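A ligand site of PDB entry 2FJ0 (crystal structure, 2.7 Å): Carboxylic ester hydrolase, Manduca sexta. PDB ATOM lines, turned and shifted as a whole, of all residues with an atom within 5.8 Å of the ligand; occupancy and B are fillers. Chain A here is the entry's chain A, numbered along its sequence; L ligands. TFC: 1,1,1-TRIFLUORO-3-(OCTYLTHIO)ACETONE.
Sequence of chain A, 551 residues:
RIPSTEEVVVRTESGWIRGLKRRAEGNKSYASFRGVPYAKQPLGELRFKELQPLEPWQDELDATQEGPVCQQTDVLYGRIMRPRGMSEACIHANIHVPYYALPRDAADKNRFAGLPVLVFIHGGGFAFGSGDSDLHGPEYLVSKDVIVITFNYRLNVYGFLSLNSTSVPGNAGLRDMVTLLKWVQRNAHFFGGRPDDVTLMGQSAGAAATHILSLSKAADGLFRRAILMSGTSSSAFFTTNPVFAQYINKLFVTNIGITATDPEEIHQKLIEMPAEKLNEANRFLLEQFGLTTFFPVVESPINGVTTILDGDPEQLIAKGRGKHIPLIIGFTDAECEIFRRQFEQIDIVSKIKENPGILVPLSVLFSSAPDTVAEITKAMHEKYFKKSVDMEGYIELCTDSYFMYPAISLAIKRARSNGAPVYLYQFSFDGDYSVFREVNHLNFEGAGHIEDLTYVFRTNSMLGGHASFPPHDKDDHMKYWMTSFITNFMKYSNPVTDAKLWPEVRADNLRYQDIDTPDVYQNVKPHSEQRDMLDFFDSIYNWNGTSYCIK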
ATOM      1  N   LEU A  76      11.168  13.438  27.068  1.00  0.00           N
ATOM      2  CA  LEU A  76      10.759  12.586  25.955  1.00  0.00           C
ATOM      3  C   LEU A  76      11.800  11.854  25.133  1.00  0.00           C
ATOM      4  O   LEU A  76      11.714  10.644  24.942  1.00  0.00           O
ATOM      5  CB  LEU A  76       9.898  13.401  24.964  1.00  0.00           C
ATOM      6  CG  LEU A  76       9.551  12.734  23.622  1.00  0.00           C
ATOM      7  CD1 LEU A  76       8.600  11.565  23.868  1.00  0.00           C
ATOM      8  CD2 LEU A  76       8.936  13.760  22.652  1.00  0.00           C
ATOM      9  N   TYR A  77      12.778  12.592  24.628  1.00  0.00           N
ATOM     10  CA  TYR A  77      13.768  12.009  23.749  1.00  0.00           C
ATOM     11  C   TYR A  77      14.648  10.984  24.361  1.00  0.00           C
ATOM     12  O   TYR A  77      15.091  10.052  23.683  1.00  0.00           O
ATOM     13  CB  TYR A  77      14.587  13.113  23.112  1.00  0.00           C
ATOM     14  CG  TYR A  77      13.709  13.990  22.264  1.00  0.00           C
ATOM     15  CD1 TYR A  77      13.319  15.257  22.707  1.00  0.00           C
ATOM     16  CD2 TYR A  77      13.233  13.544  21.024  1.00  0.00           C
ATOM     17  CE1 TYR A  77      12.467  16.058  21.938  1.00  0.00           C
ATOM     18  CE2 TYR A  77      12.393  14.346  20.245  1.00  0.00           C
ATOM     19  CZ  TYR A  77      12.020  15.598  20.708  1.00  0.00           C
ATOM     20  OH  TYR A  77      11.251  16.409  19.918  1.00  0.00           O
ATOM     21  N   GLY A 123      10.882  19.950  17.255  1.00  0.00           N
ATOM     22  CA  GLY A 123       9.782  19.783  18.186  1.00  0.00           C
ATOM     23  C   GLY A 123      10.308  19.554  19.592  1.00  0.00           C
ATOM     24  O   GLY A 123      11.507  19.684  19.859  1.00  0.00           O
ATOM     25  N   GLY A 124       9.415  19.207  20.500  1.00  0.00           N
ATOM     26  CA  GLY A 124       9.806  18.990  21.877  1.00  0.00           C
ATOM     27  C   GLY A 124       8.795  19.694  22.788  1.00  0.00           C
ATOM     28  O   GLY A 124       9.152  20.126  23.883  1.00  0.00           O
ATOM     29  N   GLY A 125       7.555  19.831  22.311  1.00  0.00           N
ATOM     30  CA  GLY A 125       6.517  20.475  23.094  1.00  0.00           C
ATOM     31  C   GLY A 125       6.771  21.907  23.547  1.00  0.00           C
ATOM     32  O   GLY A 125       6.097  22.384  24.475  1.00  0.00           O
ATOM     33  N   PHE A 126       7.709  22.606  22.899  1.00  0.00           N
ATOM     34  CA  PHE A 126       8.070  23.978  23.274  1.00  0.00           C
ATOM     35  C   PHE A 126       8.846  23.950  24.593  1.00  0.00           C
ATOM     36  O   PHE A 126       9.270  24.996  25.077  1.00  0.00           O
ATOM     37  CB  PHE A 126       6.835  24.846  23.531  1.00  0.00           C
ATOM     38  CG  PHE A 126       5.901  24.966  22.375  1.00  0.00           C
ATOM     39  CD1 PHE A 126       6.255  25.718  21.258  1.00  0.00           C
ATOM     40  CD2 PHE A 126       4.618  24.384  22.426  1.00  0.00           C
ATOM     41  CE1 PHE A 126       5.359  25.904  20.201  1.00  0.00           C
ATOM     42  CE2 PHE A 126       3.722  24.547  21.377  1.00  0.00           C
ATOM     43  CZ  PHE A 126       4.097  25.319  20.256  1.00  0.00           C
ATOM     44  N   PHE A 128      11.416  21.279  25.408  1.00  0.00           N
ATOM     45  CA  PHE A 128      12.695  20.596  25.327  1.00  0.00           C
ATOM     46  C   PHE A 128      13.047  20.277  23.891  1.00  0.00           C
ATOM     47  O   PHE A 128      12.320  20.657  22.960  1.00  0.00           O
ATOM     48  CB  PHE A 128      12.644  19.335  26.166  1.00  0.00           C
ATOM     49  CG  PHE A 128      11.372  18.560  25.975  1.00  0.00           C
ATOM     50  CD1 PHE A 128      11.246  17.640  24.942  1.00  0.00           C
ATOM     51  CD2 PHE A 128      10.272  18.786  26.827  1.00  0.00           C
ATOM     52  CE1 PHE A 128      10.029  16.946  24.738  1.00  0.00           C
ATOM     53  CE2 PHE A 128       9.064  18.105  26.635  1.00  0.00           C
ATOM     54  CZ  PHE A 128       8.938  17.190  25.580  1.00  0.00           C
ATOM     55  N   GLN A 203       8.272  20.022  13.121  1.00  0.00           N
ATOM     56  CA  GLN A 203       7.463  18.861  13.452  1.00  0.00           C
ATOM     57  C   GLN A 203       7.072  19.060  14.916  1.00  0.00           C
ATOM     58  O   GLN A 203       7.840  19.594  15.717  1.00  0.00           O
ATOM     59  CB  GLN A 203       8.190  17.528  13.130  1.00  0.00           C
ATOM     60  CG  GLN A 203       8.897  16.821  14.247  1.00  0.00           C
ATOM     61  CD  GLN A 203       7.987  15.966  15.157  1.00  0.00           C
ATOM     62  OE1 GLN A 203       7.021  15.346  14.708  1.00  0.00           O
ATOM     63  NE2 GLN A 203       8.337  15.904  16.446  1.00  0.00           N
ATOM     64  N   SER A 204       5.839  18.674  15.228  1.00  0.00           N
ATOM     65  CA  SER A 204       5.272  18.854  16.577  1.00  0.00           C
ATOM     66  C   SER A 204       5.337  20.341  16.929  1.00  0.00           C
ATOM     67  O   SER A 204       5.110  21.171  16.051  1.00  0.00           O
ATOM     68  CB  SER A 204       6.123  17.753  17.113  1.00  0.00           C
ATOM     69  OG  SER A 204       6.352  16.775  18.099  1.00  0.00           O
ATOM     70  N   ALA A 205       5.618  20.659  18.186  1.00  0.00           N
ATOM     71  CA  ALA A 205       5.702  22.068  18.574  1.00  0.00           C
ATOM     72  C   ALA A 205       6.403  22.826  17.445  1.00  0.00           C
ATOM     73  O   ALA A 205       5.959  23.922  17.046  1.00  0.00           O
ATOM     74  CB  ALA A 205       6.475  22.208  19.863  1.00  0.00           C
ATOM     75  N   GLY A 206       7.457  22.221  16.887  1.00  0.00           N
ATOM     76  CA  GLY A 206       8.192  22.845  15.795  1.00  0.00           C
ATOM     77  C   GLY A 206       7.275  23.187  14.617  1.00  0.00           C
ATOM     78  O   GLY A 206       7.345  24.292  14.064  1.00  0.00           O
ATOM     79  N   SER A 230       3.078  16.948  11.419  1.00  0.00           N
ATOM     80  CA  SER A 230       2.333  16.689  12.650  1.00  0.00           C
ATOM     81  C   SER A 230       2.310  17.874  13.620  1.00  0.00           C
ATOM     82  O   SER A 230       2.795  17.758  14.754  1.00  0.00           O
ATOM     83  CB  SER A 230       2.896  15.474  13.402  1.00  0.00           C
ATOM     84  OG  SER A 230       2.719  14.268  12.666  1.00  0.00           O
ATOM     85  N   PHE A 237      -2.915  19.947  21.303  1.00  0.00           N
ATOM     86  CA  PHE A 237      -1.949  19.546  22.311  1.00  0.00           C
ATOM     87  C   PHE A 237      -1.405  20.712  23.120  1.00  0.00           C
ATOM     88  O   PHE A 237      -0.597  20.504  24.035  1.00  0.00           O
ATOM     89  CB  PHE A 237      -0.811  18.734  21.687  1.00  0.00           C
ATOM     90  CG  PHE A 237       0.118  19.529  20.827  1.00  0.00           C
ATOM     91  CD1 PHE A 237       1.097  20.353  21.392  1.00  0.00           C
ATOM     92  CD2 PHE A 237       0.076  19.403  19.435  1.00  0.00           C
ATOM     93  CE1 PHE A 237       2.021  21.022  20.591  1.00  0.00           C
ATOM     94  CE2 PHE A 237       1.006  20.066  18.619  1.00  0.00           C
ATOM     95  CZ  PHE A 237       1.970  20.878  19.208  1.00  0.00           C
ATOM     96  N   PHE A 289       1.799  18.771  34.019  1.00  0.00           N
ATOM     97  CA  PHE A 289       1.173  18.718  32.695  1.00  0.00           C
ATOM     98  C   PHE A 289       1.650  17.572  31.779  1.00  0.00           C
ATOM     99  O   PHE A 289       1.109  17.391  30.678  1.00  0.00           O
ATOM    100  CB  PHE A 289       1.397  20.020  31.948  1.00  0.00           C
ATOM    101  CG  PHE A 289       0.830  21.205  32.625  1.00  0.00           C
ATOM    102  CD1 PHE A 289       1.668  22.147  33.199  1.00  0.00           C
ATOM    103  CD2 PHE A 289      -0.539  21.404  32.668  1.00  0.00           C
ATOM    104  CE1 PHE A 289       1.144  23.277  33.822  1.00  0.00           C
ATOM    105  CE2 PHE A 289      -1.079  22.527  33.294  1.00  0.00           C
ATOM    106  CZ  PHE A 289      -0.236  23.475  33.874  1.00  0.00           C
ATOM    107  N   GLY A 290       2.667  16.836  32.210  1.00  0.00           N
ATOM    108  CA  GLY A 290       3.139  15.739  31.392  1.00  0.00           C
ATOM    109  C   GLY A 290       4.282  16.009  30.434  1.00  0.00           C
ATOM    110  O   GLY A 290       5.448  15.731  30.773  1.00  0.00           O
ATOM    111  N   LEU A 291       3.970  16.552  29.256  1.00  0.00           N
ATOM    112  CA  LEU A 291       4.980  16.803  28.235  1.00  0.00           C
ATOM    113  C   LEU A 291       5.175  18.230  27.801  1.00  0.00           C
ATOM    114  O   LEU A 291       5.855  18.479  26.825  1.00  0.00           O
ATOM    115  CB  LEU A 291       4.656  15.991  26.984  1.00  0.00           C
ATOM    116  CG  LEU A 291       4.697  14.469  27.069  1.00  0.00           C
ATOM    117  CD1 LEU A 291       3.992  13.852  25.868  1.00  0.00           C
ATOM    118  CD2 LEU A 291       6.136  14.021  27.130  1.00  0.00           C
ATOM    119  N   THR A 292       4.545  19.175  28.487  1.00  0.00           N
ATOM    120  CA  THR A 292       4.668  20.584  28.109  1.00  0.00           C
ATOM    121  C   THR A 292       4.543  21.487  29.327  1.00  0.00           C
ATOM    122  O   THR A 292       4.085  21.058  30.385  1.00  0.00           O
ATOM    123  CB  THR A 292       3.554  21.043  27.129  1.00  0.00           C
ATOM    124  OG1 THR A 292       2.280  20.903  27.763  1.00  0.00           O
ATOM    125  CG2 THR A 292       3.557  20.246  25.853  1.00  0.00           C
ATOM    126  N   PHE A 339       3.996   7.899  22.506  1.00  0.00           N
ATOM    127  CA  PHE A 339       4.045   8.438  23.874  1.00  0.00           C
ATOM    128  C   PHE A 339       3.685   7.465  25.004  1.00  0.00           C
ATOM    129  O   PHE A 339       3.798   7.830  26.185  1.00  0.00           O
ATOM    130  CB  PHE A 339       3.097   9.645  24.001  1.00  0.00           C
ATOM    131  CG  PHE A 339       3.420  10.790  23.089  1.00  0.00           C
ATOM    132  CD1 PHE A 339       2.416  11.381  22.313  1.00  0.00           C
ATOM    133  CD2 PHE A 339       4.711  11.308  23.019  1.00  0.00           C
ATOM    134  CE1 PHE A 339       2.695  12.466  21.498  1.00  0.00           C
ATOM    135  CE2 PHE A 339       5.014  12.396  22.200  1.00  0.00           C
ATOM    136  CZ  PHE A 339       3.999  12.986  21.433  1.00  0.00           C
ATOM    137  N   PHE A 343       3.098   8.237  28.913  1.00  0.00           N
ATOM    138  CA  PHE A 343       1.710   8.303  29.375  1.00  0.00           C
ATOM    139  C   PHE A 343       1.628   7.486  30.660  1.00  0.00           C
ATOM    140  O   PHE A 343       0.973   7.885  31.624  1.00  0.00           O
ATOM    141  CB  PHE A 343       0.777   7.763  28.306  1.00  0.00           C
ATOM    142  CG  PHE A 343       0.522   8.727  27.175  1.00  0.00           C
ATOM    143  CD1 PHE A 343      -0.109   8.317  26.007  1.00  0.00           C
ATOM    144  CD2 PHE A 343       0.892  10.073  27.291  1.00  0.00           C
ATOM    145  CE1 PHE A 343      -0.371   9.231  24.951  1.00  0.00           C
ATOM    146  CE2 PHE A 343       0.646  10.988  26.254  1.00  0.00           C
ATOM    147  CZ  PHE A 343       0.004  10.560  25.082  1.00  0.00           C
ATOM    148  N   ILE A 346       3.390   9.253  33.772  1.00  0.00           N
ATOM    149  CA  ILE A 346       2.557  10.259  34.409  1.00  0.00           C
ATOM    150  C   ILE A 346       1.236   9.659  34.868  1.00  0.00           C
ATOM    151  O   ILE A 346       0.481  10.250  35.666  1.00  0.00           O
ATOM    152  CB  ILE A 346       2.278  11.448  33.462  1.00  0.00           C
ATOM    153  CG1 ILE A 346       1.283  11.045  32.388  1.00  0.00           C
ATOM    154  CG2 ILE A 346       3.569  11.897  32.793  1.00  0.00           C
ATOM    155  CD1 ILE A 346       0.793  12.232  31.597  1.00  0.00           C
ATOM    156  N   ILE A 348      -1.625   8.664  32.936  1.00  0.00           N
ATOM    157  CA  ILE A 348      -2.747   9.401  32.400  1.00  0.00           C
ATOM    158  C   ILE A 348      -4.079   8.820  32.781  1.00  0.00           C
ATOM    159  O   ILE A 348      -5.055   9.563  32.903  1.00  0.00           O
ATOM    160  CB  ILE A 348      -2.735   9.509  30.864  1.00  0.00           C
ATOM    161  CG1 ILE A 348      -1.912   8.370  30.280  1.00  0.00           C
ATOM    162  CG2 ILE A 348      -2.266  10.870  30.433  1.00  0.00           C
ATOM    163  CD1 ILE A 348      -2.526   7.007  30.490  1.00  0.00           C
ATOM    164  N   TYR A 394      -7.189   6.689  25.594  1.00  0.00           N
ATOM    165  CA  TYR A 394      -6.557   8.002  25.556  1.00  0.00           C
ATOM    166  C   TYR A 394      -5.682   8.143  24.326  1.00  0.00           C
ATOM    167  O   TYR A 394      -5.737   9.158  23.632  1.00  0.00           O
ATOM    168  CB  TYR A 394      -5.720   8.265  26.813  1.00  0.00           C
ATOM    169  CG  TYR A 394      -5.148   9.679  26.858  1.00  0.00           C
ATOM    170  CD1 TYR A 394      -6.006  10.795  26.919  1.00  0.00           C
ATOM    171  CD2 TYR A 394      -3.780   9.913  26.727  1.00  0.00           C
ATOM    172  CE1 TYR A 394      -5.511  12.096  26.846  1.00  0.00           C
ATOM    173  CE2 TYR A 394      -3.271  11.222  26.651  1.00  0.00           C
ATOM    174  CZ  TYR A 394      -4.142  12.295  26.702  1.00  0.00           C
ATOM    175  OH  TYR A 394      -3.657  13.576  26.560  1.00  0.00           O
ATOM    176  N   CYS A 398      -5.775  11.398  22.000  1.00  0.00           N
ATOM    177  CA  CYS A 398      -4.587  12.198  21.701  1.00  0.00           C
ATOM    178  C   CYS A 398      -4.268  12.228  20.207  1.00  0.00           C
ATOM    179  O   CYS A 398      -4.078  13.306  19.629  1.00  0.00           O
ATOM    180  CB  CYS A 398      -3.410  11.641  22.512  1.00  0.00           C
ATOM    181  SG  CYS A 398      -1.696  12.163  22.131  1.00  0.00           S
ATOM    182  N   TYR A 402      -5.109  15.704  18.892  1.00  0.00           N
ATOM    183  CA  TYR A 402      -3.900  16.499  18.863  1.00  0.00           C
ATOM    184  C   TYR A 402      -3.236  16.557  17.513  1.00  0.00           C
ATOM    185  O   TYR A 402      -2.494  17.503  17.234  1.00  0.00           O
ATOM    186  CB  TYR A 402      -2.891  15.982  19.899  1.00  0.00           C
ATOM    187  CG  TYR A 402      -3.402  15.997  21.321  1.00  0.00           C
ATOM    188  CD1 TYR A 402      -2.582  15.592  22.375  1.00  0.00           C
ATOM    189  CD2 TYR A 402      -4.703  16.405  21.614  1.00  0.00           C
ATOM    190  CE1 TYR A 402      -3.056  15.595  23.684  1.00  0.00           C
ATOM    191  CE2 TYR A 402      -5.192  16.406  22.904  1.00  0.00           C
ATOM    192  CZ  TYR A 402      -4.370  16.007  23.950  1.00  0.00           C
ATOM    193  OH  TYR A 402      -4.881  16.029  25.249  1.00  0.00           O
ATOM    194  N   PHE A 403      -3.504  15.569  16.657  1.00  0.00           N
ATOM    195  CA  PHE A 403      -2.818  15.564  15.393  1.00  0.00           C
ATOM    196  C   PHE A 403      -3.595  15.344  14.145  1.00  0.00           C
ATOM    197  O   PHE A 403      -3.567  16.181  13.255  1.00  0.00           O
ATOM    198  CB  PHE A 403      -1.682  14.567  15.461  1.00  0.00           C
ATOM    199  CG  PHE A 403      -0.699  14.869  16.520  1.00  0.00           C
ATOM    200  CD1 PHE A 403      -0.744  14.216  17.733  1.00  0.00           C
ATOM    201  CD2 PHE A 403       0.210  15.902  16.353  1.00  0.00           C
ATOM    202  CE1 PHE A 403       0.109  14.577  18.774  1.00  0.00           C
ATOM    203  CE2 PHE A 403       1.058  16.280  17.380  1.00  0.00           C
ATOM    204  CZ  PHE A 403       1.006  15.614  18.594  1.00  0.00           C
ATOM    205  N   HIS A 449       3.940   9.319  16.046  1.00  0.00           N
ATOM    206  CA  HIS A 449       4.442  10.687  16.011  1.00  0.00           C
ATOM    207  C   HIS A 449       5.968  10.756  15.943  1.00  0.00           C
ATOM    208  O   HIS A 449       6.656  10.045  16.669  1.00  0.00           O
ATOM    209  CB  HIS A 449       3.951  11.355  17.272  1.00  0.00           C
ATOM    210  CG  HIS A 449       4.047  12.839  17.259  1.00  0.00           C
ATOM    211  ND1 HIS A 449       3.376  13.609  16.327  1.00  0.00           N
ATOM    212  CD2 HIS A 449       4.689  13.702  18.077  1.00  0.00           C
ATOM    213  CE1 HIS A 449       3.607  14.879  16.578  1.00  0.00           C
ATOM    214  NE2 HIS A 449       4.401  14.966  17.629  1.00  0.00           N
ATOM    215  N   ILE A 450       6.491  11.630  15.079  1.00  0.00           N
ATOM    216  CA  ILE A 450       7.942  11.861  14.892  1.00  0.00           C
ATOM    217  C   ILE A 450       8.652  10.887  13.965  1.00  0.00           C
ATOM    218  O   ILE A 450       9.774  11.168  13.519  1.00  0.00           O
ATOM    219  CB  ILE A 450       8.776  11.776  16.198  1.00  0.00           C
ATOM    220  CG1 ILE A 450       8.157  12.575  17.328  1.00  0.00           C
ATOM    221  CG2 ILE A 450      10.148  12.314  15.948  1.00  0.00           C
ATOM    222  CD1 ILE A 450       8.934  12.390  18.619  1.00  0.00           C
HETATM  223  C1  TFC L   1      -0.047  14.491  28.658  1.00  0.00           C
HETATM  224  C2  TFC L   1      -0.458  14.405  27.179  1.00  0.00           C
HETATM  225  C3  TFC L   1       0.652  14.953  26.290  1.00  0.00           C
HETATM  226  C4  TFC L   1       0.334  14.767  24.802  1.00  0.00           C
HETATM  227  C5  TFC L   1       1.473  15.301  23.923  1.00  0.00           C
HETATM  228  C6  TFC L   1       1.575  16.820  24.066  1.00  0.00           C
HETATM  229  C7  TFC L   1       2.863  17.393  23.463  1.00  0.00           C
HETATM  230  C8  TFC L   1       2.968  17.211  21.943  1.00  0.00           C
HETATM  231  S1  TFC L   1       4.316  18.243  21.261  1.00  0.00           S
HETATM  232  C9  TFC L   1       4.711  17.338  19.735  1.00  0.00           C
HETATM  233  C10 TFC L   1       6.209  17.312  19.411  1.00  0.00           C
HETATM  234  O1  TFC L   1       6.689  18.668  19.438  1.00  0.00           O
HETATM  235  C11 TFC L   1       7.065  16.442  20.334  1.00  0.00           C
HETATM  236  F1  TFC L   1       8.325  16.449  19.903  1.00  0.00           F
HETATM  237  F2  TFC L   1       6.651  15.182  20.320  1.00  0.00           F
HETATM  238  F3  TFC L   1       7.041  16.875  21.590  1.00  0.00           F
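The backbone NH (N) of Gly 124 lies within hydrogen-bond range of the side-chain hydroxyl (OH) of Tyr 77, 3.4 Å away. The backbone carbonyl oxygen (O) of Gly 123 is in hydrogen-bond range of the side-chain hydroxyl (OH) of Tyr 77 (3.3 Å). The side-chain hydroxyl (OH) of Tyr 394 lies within hydrogen-bond range of the side-chain hydroxyl (OH) of Tyr 402 (3.0 Å). The backbone carbonyl oxygen (O) of Gln 203 lies close to the backbone NH (N) of Gly 123. OG of Ser 204 is in hydrogen-bond range of NE2 of Gln 203 (2.7 Å). The backbone NH (N) of Ser 204 lies within hydrogen-bond range of the backbone carbonyl oxygen (O) of Ser 230 (3.2 Å). The backbone carbonyl oxygen (O) of Phe 343 sits at hydrogen-bond distance from the backbone NH (N) of Ile 348 (3.0 Å). NE2 of His 449 is in hydrogen-bond range of OG of Ser 204 (2.7 Å).
The side-chain hydroxyl (OH) of Tyr 77 lies close to a fluorine (F1) of the ligand. NE2 of Gln 203 lies close to F1 of the ligand, 3.5 Å away. CD2 of Leu 76 touches F2 of the ligand (3.6 Å). CA of Gly 123 touches O1 of the ligand, at 3.5 Å. CE1 of Phe 237 touches S1 of the ligand, at 3.7 Å. Phe 289 touches the ligand. Leu 291 touches the ligand (CD1 to C5, 3.5 Å). Thr 292 touches the ligand. CZ of Phe 339 touches F2 of the ligand, 3.6 Å away. CE2 of Phe 343 touches C2 of the ligand, at 3.7 Å. CD1 of Ile 346 touches C1 of the ligand (3.8 Å). Tyr 394 touches the ligand. Tyr 402 touches the ligand. NE2 of His 449 touches C9 of the ligand (3.2 Å). Ile 450 touches the ligand. Of the 27 residues printed, 19 come within 4 Å of the ligand. The nearest printed residue that does not touch the ligand is Phe 403 (4.2 Å).
An oxygen (O1) of the ligand sits at hydrogen-bond distance from the backbone NH (N) of Gly 125 (3.2 Å). The backbone NH (N) of Ala 205 is in hydrogen-bond range of an oxygen (O1) of the ligand (2.6 Å). N of Gly 124 is in hydrogen-bond range of O1 of the ligand (3.0 Å). The side-chain hydroxyl (OG) of Ser 204 is bonded to a carbon (C10) of the ligand (1.4 Å).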
